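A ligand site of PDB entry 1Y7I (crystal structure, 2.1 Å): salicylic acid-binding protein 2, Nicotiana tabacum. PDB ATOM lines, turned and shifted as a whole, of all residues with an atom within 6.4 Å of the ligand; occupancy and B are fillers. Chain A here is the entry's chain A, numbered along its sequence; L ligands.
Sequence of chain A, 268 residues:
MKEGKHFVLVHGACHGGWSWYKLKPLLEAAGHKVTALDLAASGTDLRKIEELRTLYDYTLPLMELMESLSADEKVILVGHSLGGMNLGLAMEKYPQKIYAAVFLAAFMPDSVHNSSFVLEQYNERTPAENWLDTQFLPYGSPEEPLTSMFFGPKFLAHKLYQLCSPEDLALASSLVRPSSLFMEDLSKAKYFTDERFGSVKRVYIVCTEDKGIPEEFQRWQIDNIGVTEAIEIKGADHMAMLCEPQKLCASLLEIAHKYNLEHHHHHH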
ATOM      1  N   HIS A  11      22.524  16.944 -27.715  1.00  0.00           N
ATOM      2  CA  HIS A  11      21.777  17.154 -26.473  1.00  0.00           C
ATOM      3  C   HIS A  11      20.993  18.471 -26.444  1.00  0.00           C
ATOM      4  O   HIS A  11      21.218  19.367 -27.269  1.00  0.00           O
ATOM      5  CB  HIS A  11      22.764  17.119 -25.319  1.00  0.00           C
ATOM      6  CG  HIS A  11      23.725  18.275 -25.331  1.00  0.00           C
ATOM      7  ND1 HIS A  11      23.361  19.539 -24.930  1.00  0.00           N
ATOM      8  CD2 HIS A  11      25.001  18.359 -25.767  1.00  0.00           C
ATOM      9  CE1 HIS A  11      24.383  20.364 -25.119  1.00  0.00           C
ATOM     10  NE2 HIS A  11      25.389  19.672 -25.623  1.00  0.00           N
ATOM     11  N   GLY A  12      20.086  18.594 -25.474  1.00  0.00           N
ATOM     12  CA  GLY A  12      19.279  19.794 -25.324  1.00  0.00           C
ATOM     13  C   GLY A  12      19.890  20.844 -24.403  1.00  0.00           C
ATOM     14  O   GLY A  12      21.078  20.771 -24.095  1.00  0.00           O
ATOM     15  N   ALA A  13      19.097  21.803 -23.928  1.00  0.00           N
ATOM     16  CA  ALA A  13      19.638  22.846 -23.052  1.00  0.00           C
ATOM     17  C   ALA A  13      20.017  22.334 -21.659  1.00  0.00           C
ATOM     18  O   ALA A  13      19.281  21.558 -21.047  1.00  0.00           O
ATOM     19  CB  ALA A  13      18.650  23.994 -22.933  1.00  0.00           C
ATOM     20  N   CYS A  14      21.164  22.814 -21.174  1.00  0.00           N
ATOM     21  CA  CYS A  14      21.695  22.483 -19.847  1.00  0.00           C
ATOM     22  C   CYS A  14      22.255  21.077 -19.741  1.00  0.00           C
ATOM     23  O   CYS A  14      22.758  20.680 -18.688  1.00  0.00           O
ATOM     24  CB  CYS A  14      20.618  22.709 -18.791  1.00  0.00           C
ATOM     25  SG  CYS A  14      19.879  24.381 -18.841  1.00  0.00           S
ATOM     26  N   HIS A  15      22.187  20.322 -20.836  1.00  0.00           N
ATOM     27  CA  HIS A  15      22.701  18.958 -20.845  1.00  0.00           C
ATOM     28  C   HIS A  15      23.994  18.831 -21.646  1.00  0.00           C
ATOM     29  O   HIS A  15      24.569  19.843 -22.047  1.00  0.00           O
ATOM     30  CB  HIS A  15      21.615  18.022 -21.389  1.00  0.00           C
ATOM     31  CG  HIS A  15      20.539  17.720 -20.389  1.00  0.00           C
ATOM     32  ND1 HIS A  15      19.678  18.687 -19.916  1.00  0.00           N
ATOM     33  CD2 HIS A  15      20.248  16.592 -19.713  1.00  0.00           C
ATOM     34  CE1 HIS A  15      18.902  18.161 -18.993  1.00  0.00           C
ATOM     35  NE2 HIS A  15      19.222  16.881 -18.847  1.00  0.00           N
ATOM     36  N   HIS A  80      17.835  16.559 -29.527  1.00  0.00           N
ATOM     37  CA  HIS A  80      16.889  16.498 -28.417  1.00  0.00           C
ATOM     38  C   HIS A  80      16.497  17.903 -28.014  1.00  0.00           C
ATOM     39  O   HIS A  80      17.357  18.772 -27.895  1.00  0.00           O
ATOM     40  CB  HIS A  80      17.536  15.793 -27.219  1.00  0.00           C
ATOM     41  CG  HIS A  80      16.619  15.687 -26.035  1.00  0.00           C
ATOM     42  ND1 HIS A  80      17.041  15.956 -24.750  1.00  0.00           N
ATOM     43  CD2 HIS A  80      15.332  15.299 -25.936  1.00  0.00           C
ATOM     44  CE1 HIS A  80      16.048  15.733 -23.909  1.00  0.00           C
ATOM     45  NE2 HIS A  80      14.991  15.345 -24.605  1.00  0.00           N
ATOM     46  N   SER A  81      15.205  18.121 -27.796  1.00  0.00           N
ATOM     47  CA  SER A  81      14.686  19.430 -27.391  1.00  0.00           C
ATOM     48  C   SER A  81      15.334  20.614 -28.123  1.00  0.00           C
ATOM     49  O   SER A  81      15.114  20.799 -29.323  1.00  0.00           O
ATOM     50  CB  SER A  81      14.834  19.589 -25.876  1.00  0.00           C
ATOM     51  OG  SER A  81      16.162  19.303 -25.445  1.00  0.00           O
ATOM     52  N   LEU A  82      16.105  21.436 -27.406  1.00  0.00           N
ATOM     53  CA  LEU A  82      16.751  22.599 -28.008  1.00  0.00           C
ATOM     54  C   LEU A  82      17.724  22.153 -29.107  1.00  0.00           C
ATOM     55  O   LEU A  82      17.970  22.889 -30.068  1.00  0.00           O
ATOM     56  CB  LEU A  82      17.516  23.404 -26.945  1.00  0.00           C
ATOM     57  CG  LEU A  82      18.154  24.716 -27.427  1.00  0.00           C
ATOM     58  CD1 LEU A  82      17.058  25.677 -27.839  1.00  0.00           C
ATOM     59  CD2 LEU A  82      18.986  25.332 -26.299  1.00  0.00           C
ATOM     60  N   GLY A  83      18.254  20.944 -28.970  1.00  0.00           N
ATOM     61  CA  GLY A  83      19.166  20.421 -29.963  1.00  0.00           C
ATOM     62  C   GLY A  83      18.559  20.505 -31.358  1.00  0.00           C
ATOM     63  O   GLY A  83      19.270  20.466 -32.352  1.00  0.00           O
ATOM     64  N   PHE A 107      12.619  21.169 -30.511  1.00  0.00           N
ATOM     65  CA  PHE A 107      12.066  22.408 -31.010  1.00  0.00           C
ATOM     66  C   PHE A 107      12.537  22.299 -32.456  1.00  0.00           C
ATOM     67  O   PHE A 107      13.745  22.354 -32.736  1.00  0.00           O
ATOM     68  CB  PHE A 107      12.678  23.624 -30.300  1.00  0.00           C
ATOM     69  CG  PHE A 107      12.058  23.918 -28.967  1.00  0.00           C
ATOM     70  CD1 PHE A 107      12.844  23.987 -27.829  1.00  0.00           C
ATOM     71  CD2 PHE A 107      10.684  24.105 -28.842  1.00  0.00           C
ATOM     72  CE1 PHE A 107      12.267  24.240 -26.575  1.00  0.00           C
ATOM     73  CE2 PHE A 107      10.104  24.364 -27.594  1.00  0.00           C
ATOM     74  CZ  PHE A 107      10.900  24.430 -26.466  1.00  0.00           C
ATOM     75  N   LEU A 119      10.134  28.807 -30.862  1.00  0.00           N
ATOM     76  CA  LEU A 119      10.467  29.162 -29.491  1.00  0.00           C
ATOM     77  C   LEU A 119       9.503  30.210 -28.959  1.00  0.00           C
ATOM     78  O   LEU A 119       9.101  30.160 -27.795  1.00  0.00           O
ATOM     79  CB  LEU A 119      11.908  29.669 -29.404  1.00  0.00           C
ATOM     80  CG  LEU A 119      12.965  28.607 -29.745  1.00  0.00           C
ATOM     81  CD1 LEU A 119      14.378  29.201 -29.647  1.00  0.00           C
ATOM     82  CD2 LEU A 119      12.827  27.436 -28.787  1.00  0.00           C
ATOM     83  N   TYR A 122       6.132  28.584 -28.102  1.00  0.00           N
ATOM     84  CA  TYR A 122       6.279  27.827 -26.857  1.00  0.00           C
ATOM     85  C   TYR A 122       6.247  28.751 -25.633  1.00  0.00           C
ATOM     86  O   TYR A 122       5.538  28.492 -24.662  1.00  0.00           O
ATOM     87  CB  TYR A 122       7.592  27.039 -26.867  1.00  0.00           C
ATOM     88  CG  TYR A 122       7.885  26.322 -25.570  1.00  0.00           C
ATOM     89  CD1 TYR A 122       7.207  25.151 -25.213  1.00  0.00           C
ATOM     90  CD2 TYR A 122       8.842  26.818 -24.686  1.00  0.00           C
ATOM     91  CE1 TYR A 122       7.472  24.502 -23.999  1.00  0.00           C
ATOM     92  CE2 TYR A 122       9.113  26.180 -23.480  1.00  0.00           C
ATOM     93  CZ  TYR A 122       8.424  25.028 -23.143  1.00  0.00           C
ATOM     94  OH  TYR A 122       8.697  24.413 -21.944  1.00  0.00           O
ATOM     95  N   TRP A 131       8.004  27.150 -15.285  1.00  0.00           N
ATOM     96  CA  TRP A 131       9.455  27.021 -15.289  1.00  0.00           C
ATOM     97  C   TRP A 131       9.992  26.667 -13.912  1.00  0.00           C
ATOM     98  O   TRP A 131      11.183  26.414 -13.752  1.00  0.00           O
ATOM     99  CB  TRP A 131      10.114  28.296 -15.788  1.00  0.00           C
ATOM    100  CG  TRP A 131       9.899  28.553 -17.234  1.00  0.00           C
ATOM    101  CD1 TRP A 131       8.978  29.393 -17.797  1.00  0.00           C
ATOM    102  CD2 TRP A 131      10.665  28.006 -18.308  1.00  0.00           C
ATOM    103  NE1 TRP A 131       9.130  29.412 -19.160  1.00  0.00           N
ATOM    104  CE2 TRP A 131      10.162  28.573 -19.508  1.00  0.00           C
ATOM    105  CE3 TRP A 131      11.738  27.102 -18.381  1.00  0.00           C
ATOM    106  CZ2 TRP A 131      10.684  28.264 -20.758  1.00  0.00           C
ATOM    107  CZ3 TRP A 131      12.260  26.793 -19.632  1.00  0.00           C
ATOM    108  CH2 TRP A 131      11.735  27.375 -20.806  1.00  0.00           C
ATOM    109  N   MET A 149      19.667  30.660 -19.205  1.00  0.00           N
ATOM    110  CA  MET A 149      18.652  29.748 -18.671  1.00  0.00           C
ATOM    111  C   MET A 149      19.281  28.529 -18.014  1.00  0.00           C
ATOM    112  O   MET A 149      19.953  27.731 -18.671  1.00  0.00           O
ATOM    113  CB  MET A 149      17.707  29.311 -19.789  1.00  0.00           C
ATOM    114  CG  MET A 149      16.714  28.240 -19.378  1.00  0.00           C
ATOM    115  SD  MET A 149      15.639  27.699 -20.872  1.00  0.00           S
ATOM    116  CE  MET A 149      16.884  26.521 -21.754  1.00  0.00           C
ATOM    117  N   PHE A 151      18.246  25.270 -15.645  1.00  0.00           N
ATOM    118  CA  PHE A 151      17.220  24.447 -15.003  1.00  0.00           C
ATOM    119  C   PHE A 151      17.545  24.130 -13.539  1.00  0.00           C
ATOM    120  O   PHE A 151      18.671  23.751 -13.215  1.00  0.00           O
ATOM    121  CB  PHE A 151      17.019  23.117 -15.740  1.00  0.00           C
ATOM    122  CG  PHE A 151      16.628  23.262 -17.189  1.00  0.00           C
ATOM    123  CD1 PHE A 151      15.883  24.350 -17.615  1.00  0.00           C
ATOM    124  CD2 PHE A 151      17.004  22.307 -18.114  1.00  0.00           C
ATOM    125  CE1 PHE A 151      15.516  24.483 -18.953  1.00  0.00           C
ATOM    126  CE2 PHE A 151      16.642  22.421 -19.460  1.00  0.00           C
ATOM    127  CZ  PHE A 151      15.900  23.509 -19.873  1.00  0.00           C
ATOM    128  N   PHE A 155      12.391  21.816 -11.405  1.00  0.00           N
ATOM    129  CA  PHE A 155      12.000  21.802 -12.801  1.00  0.00           C
ATOM    130  C   PHE A 155      12.448  20.485 -13.431  1.00  0.00           C
ATOM    131  O   PHE A 155      11.693  19.857 -14.162  1.00  0.00           O
ATOM    132  CB  PHE A 155      12.636  22.982 -13.545  1.00  0.00           C
ATOM    133  CG  PHE A 155      12.239  23.080 -14.992  1.00  0.00           C
ATOM    134  CD1 PHE A 155      13.095  22.650 -15.998  1.00  0.00           C
ATOM    135  CD2 PHE A 155      10.989  23.583 -15.354  1.00  0.00           C
ATOM    136  CE1 PHE A 155      12.729  22.717 -17.342  1.00  0.00           C
ATOM    137  CE2 PHE A 155      10.600  23.650 -16.702  1.00  0.00           C
ATOM    138  CZ  PHE A 155      11.471  23.217 -17.689  1.00  0.00           C
ATOM    139  N   LEU A 160      11.026  17.433 -16.463  1.00  0.00           N
ATOM    140  CA  LEU A 160      11.805  16.662 -17.420  1.00  0.00           C
ATOM    141  C   LEU A 160      12.102  15.188 -17.123  1.00  0.00           C
ATOM    142  O   LEU A 160      12.243  14.385 -18.045  1.00  0.00           O
ATOM    143  CB  LEU A 160      13.121  17.379 -17.674  1.00  0.00           C
ATOM    144  CG  LEU A 160      13.057  18.890 -17.862  1.00  0.00           C
ATOM    145  CD1 LEU A 160      14.434  19.416 -18.202  1.00  0.00           C
ATOM    146  CD2 LEU A 160      12.059  19.233 -18.963  1.00  0.00           C
ATOM    147  N   SER A 180      20.965  28.774 -22.892  1.00  0.00           N
ATOM    148  CA  SER A 180      20.209  29.927 -23.368  1.00  0.00           C
ATOM    149  C   SER A 180      19.337  29.524 -24.549  1.00  0.00           C
ATOM    150  O   SER A 180      19.617  28.542 -25.227  1.00  0.00           O
ATOM    151  CB  SER A 180      21.157  31.051 -23.808  1.00  0.00           C
ATOM    152  OG  SER A 180      20.423  32.154 -24.315  1.00  0.00           O
ATOM    153  N   LEU A 181      18.277  30.288 -24.784  1.00  0.00           N
ATOM    154  CA  LEU A 181      17.387  30.004 -25.900  1.00  0.00           C
ATOM    155  C   LEU A 181      17.768  30.870 -27.104  1.00  0.00           C
ATOM    156  O   LEU A 181      17.232  30.690 -28.198  1.00  0.00           O
ATOM    157  CB  LEU A 181      15.941  30.266 -25.497  1.00  0.00           C
ATOM    158  CG  LEU A 181      15.323  29.355 -24.438  1.00  0.00           C
ATOM    159  CD1 LEU A 181      13.897  29.788 -24.193  1.00  0.00           C
ATOM    160  CD2 LEU A 181      15.374  27.882 -24.894  1.00  0.00           C
ATOM    161  N   GLY A 212       7.924  18.821 -20.090  1.00  0.00           N
ATOM    162  CA  GLY A 212       8.706  20.023 -20.351  1.00  0.00           C
ATOM    163  C   GLY A 212       8.182  20.676 -21.620  1.00  0.00           C
ATOM    164  O   GLY A 212       7.844  21.855 -21.646  1.00  0.00           O
ATOM    165  N   ILE A 213       8.120  19.862 -22.672  1.00  0.00           N
ATOM    166  CA  ILE A 213       7.607  20.288 -23.960  1.00  0.00           C
ATOM    167  C   ILE A 213       6.450  19.313 -24.147  1.00  0.00           C
ATOM    168  O   ILE A 213       6.635  18.192 -24.612  1.00  0.00           O
ATOM    169  CB  ILE A 213       8.664  20.094 -25.064  1.00  0.00           C
ATOM    170  CG1 ILE A 213       9.858  21.010 -24.789  1.00  0.00           C
ATOM    171  CG2 ILE A 213       8.074  20.429 -26.416  1.00  0.00           C
ATOM    172  CD1 ILE A 213      11.052  20.743 -25.693  1.00  0.00           C
ATOM    173  N   HIS A 238      10.170  13.627 -20.997  1.00  0.00           N
ATOM    174  CA  HIS A 238      11.068  14.444 -21.817  1.00  0.00           C
ATOM    175  C   HIS A 238      12.391  13.770 -22.140  1.00  0.00           C
ATOM    176  O   HIS A 238      12.916  13.935 -23.242  1.00  0.00           O
ATOM    177  CB  HIS A 238      11.379  15.776 -21.121  1.00  0.00           C
ATOM    178  CG  HIS A 238      12.143  16.743 -21.978  1.00  0.00           C
ATOM    179  ND1 HIS A 238      11.607  17.318 -23.107  1.00  0.00           N
ATOM    180  CD2 HIS A 238      13.370  17.286 -21.818  1.00  0.00           C
ATOM    181  CE1 HIS A 238      12.472  18.185 -23.607  1.00  0.00           C
ATOM    182  NE2 HIS A 238      13.544  18.195 -22.842  1.00  0.00           N
ATOM    183  N   MET A 239      12.934  13.018 -21.189  1.00  0.00           N
ATOM    184  CA  MET A 239      14.213  12.337 -21.360  1.00  0.00           C
ATOM    185  C   MET A 239      14.118  10.914 -21.870  1.00  0.00           C
ATOM    186  O   MET A 239      14.489   9.965 -21.172  1.00  0.00           O
ATOM    187  CB  MET A 239      14.972  12.314 -20.015  1.00  0.00           C
ATOM    188  CG  MET A 239      15.050  13.648 -19.298  1.00  0.00           C
ATOM    189  SD  MET A 239      15.841  15.051 -20.355  1.00  0.00           S
ATOM    190  CE  MET A 239      17.668  14.418 -20.437  1.00  0.00           C
HETATM  191  C1  LIG L   1      15.385  21.478 -23.171  1.00  0.00           C
HETATM  192  O1  LIG L   1      15.394  20.250 -22.690  1.00  0.00           O
HETATM  193  O2  LIG L   1      16.307  21.880 -23.887  1.00  0.00           O
HETATM  194  C2  LIG L   1      14.221  22.331 -22.814  1.00  0.00           C
HETATM  195  C3  LIG L   1      14.156  23.682 -23.309  1.00  0.00           C
HETATM  196  C4  LIG L   1      13.066  24.494 -22.972  1.00  0.00           C
HETATM  197  C5  LIG L   1      12.034  24.005 -22.148  1.00  0.00           C
HETATM  198  C6  LIG L   1      12.071  22.675 -21.649  1.00  0.00           C
HETATM  199  C7  LIG L   1      13.151  21.859 -21.984  1.00  0.00           C
HETATM  200  O3  LIG L   1      15.112  24.219 -24.106  1.00  0.00           O
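O1 of the ligand lies within hydrogen-bond range of NE2 of His 238 (2.8 Å).
The backbone NH (N) of Ala 13 lies within hydrogen-bond range of an oxygen (O2) of the ligand (2.8 Å).
OG of Ser 81 sits at hydrogen-bond distance from O1 of the ligand (3.0 Å).
O of His 238 lies within hydrogen-bond range of NE2 of His 80 (2.9 Å).
A ring nitrogen (ND1) of His 15 lies within hydrogen-bond range of the backbone carbonyl oxygen of Ala 13 (3.1 Å).
The backbone carbonyl oxygen (O) of Ser 81 is in hydrogen-bond range of the backbone NH (N) of Phe 107 (2.8 Å).
OH of Tyr 122 is in hydrogen-bond range of O of Gly 212 (2.7 Å).
N of Phe 151 sits close to SG of Cys 14 (3.7 Å).
O of Met 149 lies within hydrogen-bond range of SG of Cys 14 (3.4 Å).
Gly 12 touches the ligand (C to O2, 3.8 Å).
Leu 82 touches the ligand (N to O2, 3.6 Å).
Phe 107 touches the ligand.
Tyr 122 touches the ligand.
Trp 131 touches the ligand.
CE of Met 149 touches O3 of the ligand, 3.7 Å away.
Phe 151 touches the ligand (CZ to C2, 3.6 Å).
Leu 181 touches the ligand (CD2 to O3, 3.8 Å).
The nearest printed residue that does not touch the ligand is Phe 155 (4.04 Å).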
